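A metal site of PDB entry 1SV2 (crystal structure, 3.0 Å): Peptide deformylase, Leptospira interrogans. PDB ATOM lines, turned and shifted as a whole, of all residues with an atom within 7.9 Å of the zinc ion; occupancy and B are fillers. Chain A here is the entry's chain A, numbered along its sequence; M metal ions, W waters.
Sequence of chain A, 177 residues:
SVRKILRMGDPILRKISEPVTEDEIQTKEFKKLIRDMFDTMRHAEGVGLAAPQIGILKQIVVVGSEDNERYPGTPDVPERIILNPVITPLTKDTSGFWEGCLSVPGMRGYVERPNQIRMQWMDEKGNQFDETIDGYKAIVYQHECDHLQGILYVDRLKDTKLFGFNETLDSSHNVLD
NE2 of His 147 sits close to NE2 of Gln 53 (3.2 Å). A ring nitrogen (ND1) of His 143 is in hydrogen-bond range of the side-chain carboxylate of Glu 99, at 2.6 Å. N of Ser 103 lies close to SG of Cys 101 (3.2 Å). OE1 of Glu 144 sits at hydrogen-bond distance from NE2 of Gln 53, 3.2 Å away. The side-chain hydroxyl (OG) of Ser 103 lies within hydrogen-bond range of the side-chain amide oxygen (OE1) of Gln 53. The side-chain amide nitrogen (NE2) of Gln 53 sits close to the backbone NH (N) of Ala 50, 2.9 Å away.
Residues that only touch the zinc ion: Gln 53 (3.8 Å) and Glu 144 (3.8 Å). Of the 22 residues printed, 5 come within 4 Å of the zinc ion. The nearest printed residue that does not touch the zinc ion is Leu 102 (4.4 Å).
The zinc ion is bound by water W1 (2.1 Å), NE2 of His 147 (2.1 Å), NE2 of His 143 (2.2 Å) and SG of Cys 101 (2.3 Å). The zinc ion has four donor atoms within binding distance.
Water W1 bridges OE1 of Glu 144 (2.9 Å) and OE1 of Gln 53 (2.9 Å).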
ATOM      1  N   ILE A   5       3.283  31.190 -31.969  1.00  0.00           N
ATOM      2  CA  ILE A   5       3.300  30.669 -30.608  1.00  0.00           C
ATOM      3  C   ILE A   5       3.915  29.268 -30.605  1.00  0.00           C
ATOM      4  O   ILE A   5       3.430  28.369 -31.299  1.00  0.00           O
ATOM      5  CB  ILE A   5       1.869  30.578 -30.045  1.00  0.00           C
ATOM      6  CG1 ILE A   5       1.208  31.953 -30.095  1.00  0.00           C
ATOM      7  CG2 ILE A   5       1.909  30.061 -28.621  1.00  0.00           C
ATOM      8  CD1 ILE A   5      -0.175  31.990 -29.457  1.00  0.00           C
ATOM      9  N   LEU A  13      10.181  26.528 -24.005  1.00  0.00           N
ATOM     10  CA  LEU A  13       9.119  26.513 -23.008  1.00  0.00           C
ATOM     11  C   LEU A  13       9.528  25.886 -21.695  1.00  0.00           C
ATOM     12  O   LEU A  13       8.755  25.898 -20.751  1.00  0.00           O
ATOM     13  CB  LEU A  13       7.899  25.779 -23.535  1.00  0.00           C
ATOM     14  CG  LEU A  13       7.240  26.366 -24.788  1.00  0.00           C
ATOM     15  CD1 LEU A  13       6.135  25.451 -25.266  1.00  0.00           C
ATOM     16  CD2 LEU A  13       6.696  27.744 -24.489  1.00  0.00           C
ATOM     17  N   GLY A  48      -4.264  35.056 -21.656  1.00  0.00           N
ATOM     18  CA  GLY A  48      -2.998  35.594 -21.222  1.00  0.00           C
ATOM     19  C   GLY A  48      -1.910  35.016 -22.089  1.00  0.00           C
ATOM     20  O   GLY A  48      -2.153  34.066 -22.822  1.00  0.00           O
ATOM     21  N   LEU A  49      -0.719  35.598 -22.027  1.00  0.00           N
ATOM     22  CA  LEU A  49       0.412  35.117 -22.826  1.00  0.00           C
ATOM     23  C   LEU A  49       1.729  35.499 -22.177  1.00  0.00           C
ATOM     24  O   LEU A  49       1.895  36.628 -21.738  1.00  0.00           O
ATOM     25  CB  LEU A  49       0.373  35.703 -24.239  1.00  0.00           C
ATOM     26  CG  LEU A  49       1.431  35.140 -25.185  1.00  0.00           C
ATOM     27  CD1 LEU A  49       1.078  33.702 -25.498  1.00  0.00           C
ATOM     28  CD2 LEU A  49       1.496  35.957 -26.472  1.00  0.00           C
ATOM     29  N   ALA A  50       2.654  34.550 -22.120  1.00  0.00           N
ATOM     30  CA  ALA A  50       3.945  34.811 -21.528  1.00  0.00           C
ATOM     31  C   ALA A  50       4.985  34.885 -22.640  1.00  0.00           C
ATOM     32  O   ALA A  50       4.943  34.114 -23.593  1.00  0.00           O
ATOM     33  CB  ALA A  50       4.308  33.722 -20.532  1.00  0.00           C
ATOM     34  N   GLN A  53       6.360  32.023 -24.659  1.00  0.00           N
ATOM     35  CA  GLN A  53       5.458  31.302 -25.531  1.00  0.00           C
ATOM     36  C   GLN A  53       5.728  31.702 -26.980  1.00  0.00           C
ATOM     37  O   GLN A  53       5.351  30.992 -27.909  1.00  0.00           O
ATOM     38  CB  GLN A  53       3.992  31.580 -25.167  1.00  0.00           C
ATOM     39  CG  GLN A  53       3.612  31.018 -23.791  1.00  0.00           C
ATOM     40  CD  GLN A  53       2.108  31.080 -23.507  1.00  0.00           C
ATOM     41  OE1 GLN A  53       1.302  30.447 -24.192  1.00  0.00           O
ATOM     42  NE2 GLN A  53       1.736  31.840 -22.486  1.00  0.00           N
ATOM     43  N   ARG A  70     -12.832  30.945 -25.977  1.00  0.00           N
ATOM     44  CA  ARG A  70     -12.158  29.716 -25.544  1.00  0.00           C
ATOM     45  C   ARG A  70     -12.580  29.238 -24.153  1.00  0.00           C
ATOM     46  O   ARG A  70     -12.856  28.062 -23.977  1.00  0.00           O
ATOM     47  CB  ARG A  70     -10.640  29.884 -25.596  1.00  0.00           C
ATOM     48  CG  ARG A  70     -10.092  30.064 -27.013  1.00  0.00           C
ATOM     49  CD  ARG A  70      -8.574  30.087 -27.022  1.00  0.00           C
ATOM     50  NE  ARG A  70      -7.992  28.822 -26.608  1.00  0.00           N
ATOM     51  CZ  ARG A  70      -7.088  28.675 -25.639  1.00  0.00           C
ATOM     52  NH1 ARG A  70      -6.664  29.742 -24.962  1.00  0.00           N
ATOM     53  NH2 ARG A  70      -6.589  27.471 -25.343  1.00  0.00           N
ATOM     54  N   TYR A  71     -12.631  30.135 -23.180  1.00  0.00           N
ATOM     55  CA  TYR A  71     -13.037  29.768 -21.831  1.00  0.00           C
ATOM     56  C   TYR A  71     -14.280  30.583 -21.493  1.00  0.00           C
ATOM     57  O   TYR A  71     -14.285  31.372 -20.551  1.00  0.00           O
ATOM     58  CB  TYR A  71     -11.924  30.056 -20.835  1.00  0.00           C
ATOM     59  CG  TYR A  71     -10.609  29.489 -21.280  1.00  0.00           C
ATOM     60  CD1 TYR A  71      -9.774  30.207 -22.134  1.00  0.00           C
ATOM     61  CD2 TYR A  71     -10.234  28.193 -20.931  1.00  0.00           C
ATOM     62  CE1 TYR A  71      -8.590  29.655 -22.632  1.00  0.00           C
ATOM     63  CE2 TYR A  71      -9.057  27.621 -21.418  1.00  0.00           C
ATOM     64  CZ  TYR A  71      -8.236  28.358 -22.270  1.00  0.00           C
ATOM     65  OH  TYR A  71      -7.074  27.796 -22.764  1.00  0.00           O
ATOM     66  N   GLU A  99      -7.952  24.028 -17.120  1.00  0.00           N
ATOM     67  CA  GLU A  99      -7.028  24.890 -17.831  1.00  0.00           C
ATOM     68  C   GLU A  99      -6.695  24.438 -19.259  1.00  0.00           C
ATOM     69  O   GLU A  99      -6.820  23.265 -19.631  1.00  0.00           O
ATOM     70  CB  GLU A  99      -5.725  25.041 -17.011  1.00  0.00           C
ATOM     71  CG  GLU A  99      -5.797  26.106 -15.930  1.00  0.00           C
ATOM     72  CD  GLU A  99      -4.514  26.235 -15.126  1.00  0.00           C
ATOM     73  OE1 GLU A  99      -3.406  26.326 -15.716  1.00  0.00           O
ATOM     74  OE2 GLU A  99      -4.607  26.263 -13.888  1.00  0.00           O
ATOM     75  N   GLY A 100      -6.274  25.416 -20.053  1.00  0.00           N
ATOM     76  CA  GLY A 100      -5.874  25.187 -21.423  1.00  0.00           C
ATOM     77  C   GLY A 100      -4.694  26.110 -21.675  1.00  0.00           C
ATOM     78  O   GLY A 100      -4.462  27.026 -20.887  1.00  0.00           O
ATOM     79  N   CYS A 101      -3.949  25.879 -22.749  1.00  0.00           N
ATOM     80  CA  CYS A 101      -2.806  26.723 -23.058  1.00  0.00           C
ATOM     81  C   CYS A 101      -2.708  26.822 -24.562  1.00  0.00           C
ATOM     82  O   CYS A 101      -2.971  25.858 -25.268  1.00  0.00           O
ATOM     83  CB  CYS A 101      -1.521  26.121 -22.502  1.00  0.00           C
ATOM     84  SG  CYS A 101      -0.002  27.018 -22.955  1.00  0.00           S
ATOM     85  N   LEU A 102      -2.309  27.986 -25.056  1.00  0.00           N
ATOM     86  CA  LEU A 102      -2.172  28.149 -26.500  1.00  0.00           C
ATOM     87  C   LEU A 102      -0.985  27.326 -27.000  1.00  0.00           C
ATOM     88  O   LEU A 102      -0.927  26.972 -28.181  1.00  0.00           O
ATOM     89  CB  LEU A 102      -1.984  29.630 -26.853  1.00  0.00           C
ATOM     90  CG  LEU A 102      -3.173  30.533 -26.560  1.00  0.00           C
ATOM     91  CD1 LEU A 102      -2.783  31.974 -26.796  1.00  0.00           C
ATOM     92  CD2 LEU A 102      -4.347  30.143 -27.435  1.00  0.00           C
ATOM     93  N   SER A 103      -0.037  27.029 -26.111  1.00  0.00           N
ATOM     94  CA  SER A 103       1.135  26.238 -26.481  1.00  0.00           C
ATOM     95  C   SER A 103       0.799  24.758 -26.435  1.00  0.00           C
ATOM     96  O   SER A 103       1.630  23.915 -26.788  1.00  0.00           O
ATOM     97  CB  SER A 103       2.308  26.540 -25.539  1.00  0.00           C
ATOM     98  OG  SER A 103       2.774  27.867 -25.685  1.00  0.00           O
ATOM     99  N   VAL A 104      -0.416  24.449 -25.973  1.00  0.00           N
ATOM    100  CA  VAL A 104      -0.884  23.081 -25.876  1.00  0.00           C
ATOM    101  C   VAL A 104      -2.271  23.058 -26.508  1.00  0.00           C
ATOM    102  O   VAL A 104      -3.274  22.859 -25.829  1.00  0.00           O
ATOM    103  CB  VAL A 104      -0.957  22.605 -24.404  1.00  0.00           C
ATOM    104  CG1 VAL A 104      -1.494  21.187 -24.337  1.00  0.00           C
ATOM    105  CG2 VAL A 104       0.411  22.651 -23.781  1.00  0.00           C
ATOM    106  N   ARG A 113      -5.187  24.932  -8.197  1.00  0.00           N
ATOM    107  CA  ARG A 113      -4.179  25.859  -7.716  1.00  0.00           C
ATOM    108  C   ARG A 113      -4.788  26.621  -6.549  1.00  0.00           C
ATOM    109  O   ARG A 113      -6.013  26.689  -6.407  1.00  0.00           O
ATOM    110  CB  ARG A 113      -3.785  26.845  -8.814  1.00  0.00           C
ATOM    111  CG  ARG A 113      -3.258  26.225 -10.099  1.00  0.00           C
ATOM    112  CD  ARG A 113      -3.065  27.308 -11.159  1.00  0.00           C
ATOM    113  NE  ARG A 113      -2.677  26.837 -12.487  1.00  0.00           N
ATOM    114  CZ  ARG A 113      -1.425  26.670 -12.897  1.00  0.00           C
ATOM    115  NH1 ARG A 113      -0.413  26.942 -12.089  1.00  0.00           N
ATOM    116  NH2 ARG A 113      -1.194  26.240 -14.140  1.00  0.00           N
ATOM    117  N   HIS A 143      -0.957  30.412 -13.746  1.00  0.00           N
ATOM    118  CA  HIS A 143      -0.728  29.666 -14.987  1.00  0.00           C
ATOM    119  C   HIS A 143       0.344  30.387 -15.793  1.00  0.00           C
ATOM    120  O   HIS A 143       1.339  29.777 -16.193  1.00  0.00           O
ATOM    121  CB  HIS A 143      -2.000  29.606 -15.852  1.00  0.00           C
ATOM    122  CG  HIS A 143      -1.782  29.006 -17.216  1.00  0.00           C
ATOM    123  ND1 HIS A 143      -2.183  27.732 -17.583  1.00  0.00           N
ATOM    124  CD2 HIS A 143      -1.216  29.536 -18.331  1.00  0.00           C
ATOM    125  CE1 HIS A 143      -1.861  27.544 -18.871  1.00  0.00           C
ATOM    126  NE2 HIS A 143      -1.259  28.599 -19.400  1.00  0.00           N
ATOM    127  N   GLU A 144       0.131  31.679 -16.025  1.00  0.00           N
ATOM    128  CA  GLU A 144       1.059  32.464 -16.820  1.00  0.00           C
ATOM    129  C   GLU A 144       2.421  32.725 -16.189  1.00  0.00           C
ATOM    130  O   GLU A 144       3.404  32.869 -16.901  1.00  0.00           O
ATOM    131  CB  GLU A 144       0.405  33.784 -17.227  1.00  0.00           C
ATOM    132  CG  GLU A 144       0.148  33.876 -18.727  1.00  0.00           C
ATOM    133  CD  GLU A 144      -0.824  32.813 -19.250  1.00  0.00           C
ATOM    134  OE1 GLU A 144      -0.509  32.172 -20.288  1.00  0.00           O
ATOM    135  OE2 GLU A 144      -1.894  32.626 -18.631  1.00  0.00           O
ATOM    136  N   ASP A 146       3.960  30.641 -14.361  1.00  0.00           N
ATOM    137  CA  ASP A 146       4.645  29.356 -14.424  1.00  0.00           C
ATOM    138  C   ASP A 146       5.526  29.281 -15.674  1.00  0.00           C
ATOM    139  O   ASP A 146       6.656  28.783 -15.616  1.00  0.00           O
ATOM    140  CB  ASP A 146       3.612  28.213 -14.428  1.00  0.00           C
ATOM    141  CG  ASP A 146       3.274  27.707 -13.034  1.00  0.00           C
ATOM    142  OD1 ASP A 146       2.288  26.958 -12.894  1.00  0.00           O
ATOM    143  OD2 ASP A 146       3.997  28.060 -12.079  1.00  0.00           O
ATOM    144  N   HIS A 147       5.001  29.774 -16.796  1.00  0.00           N
ATOM    145  CA  HIS A 147       5.729  29.771 -18.061  1.00  0.00           C
ATOM    146  C   HIS A 147       7.111  30.374 -17.830  1.00  0.00           C
ATOM    147  O   HIS A 147       8.108  29.932 -18.406  1.00  0.00           O
ATOM    148  CB  HIS A 147       4.977  30.597 -19.115  1.00  0.00           C
ATOM    149  CG  HIS A 147       3.826  29.868 -19.779  1.00  0.00           C
ATOM    150  ND1 HIS A 147       3.964  28.694 -20.482  1.00  0.00           N
ATOM    151  CD2 HIS A 147       2.517  30.196 -19.859  1.00  0.00           C
ATOM    152  CE1 HIS A 147       2.752  28.339 -20.965  1.00  0.00           C
ATOM    153  NE2 HIS A 147       1.830  29.215 -20.620  1.00  0.00           N
ATOM    154  N   ILE A 151       7.431  26.000 -16.775  1.00  0.00           N
ATOM    155  CA  ILE A 151       6.402  25.053 -16.363  1.00  0.00           C
ATOM    156  C   ILE A 151       5.096  25.182 -17.139  1.00  0.00           C
ATOM    157  O   ILE A 151       4.531  26.268 -17.248  1.00  0.00           O
ATOM    158  CB  ILE A 151       6.086  25.219 -14.875  1.00  0.00           C
ATOM    159  CG1 ILE A 151       7.376  25.049 -14.067  1.00  0.00           C
ATOM    160  CG2 ILE A 151       5.026  24.219 -14.445  1.00  0.00           C
ATOM    161  CD1 ILE A 151       7.206  25.305 -12.601  1.00  0.00           C
ATOM    162  N   LEU A 152       4.609  24.057 -17.659  1.00  0.00           N
ATOM    163  CA  LEU A 152       3.352  24.048 -18.406  1.00  0.00           C
ATOM    164  C   LEU A 152       2.308  23.419 -17.505  1.00  0.00           C
ATOM    165  O   LEU A 152       2.651  22.658 -16.609  1.00  0.00           O
ATOM    166  CB  LEU A 152       3.495  23.252 -19.694  1.00  0.00           C
ATOM    167  CG  LEU A 152       4.616  23.719 -20.628  1.00  0.00           C
ATOM    168  CD1 LEU A 152       4.443  23.016 -21.966  1.00  0.00           C
ATOM    169  CD2 LEU A 152       4.573  25.245 -20.817  1.00  0.00           C
ATOM    170  N   TYR A 153       1.027  23.719 -17.733  1.00  0.00           N
ATOM    171  CA  TYR A 153      -0.014  23.162 -16.875  1.00  0.00           C
ATOM    172  C   TYR A 153      -0.115  21.636 -16.871  1.00  0.00           C
ATOM    173  O   TYR A 153      -0.592  21.041 -15.896  1.00  0.00           O
ATOM    174  CB  TYR A 153      -1.366  23.788 -17.233  1.00  0.00           C
ATOM    175  CG  TYR A 153      -2.047  23.196 -18.438  1.00  0.00           C
ATOM    176  CD1 TYR A 153      -2.995  22.189 -18.300  1.00  0.00           C
ATOM    177  CD2 TYR A 153      -1.773  23.672 -19.713  1.00  0.00           C
ATOM    178  CE1 TYR A 153      -3.657  21.659 -19.409  1.00  0.00           C
ATOM    179  CE2 TYR A 153      -2.420  23.158 -20.830  1.00  0.00           C
ATOM    180  CZ  TYR A 153      -3.368  22.148 -20.670  1.00  0.00           C
ATOM    181  OH  TYR A 153      -4.033  21.655 -21.775  1.00  0.00           O
HETATM  182 ZN    ZN M   1      -0.075  28.511 -21.266  1.00  0.00          ZN
HETATM  183  O   HOH W   1      -0.894  30.177 -22.297  1.00  0.00           O
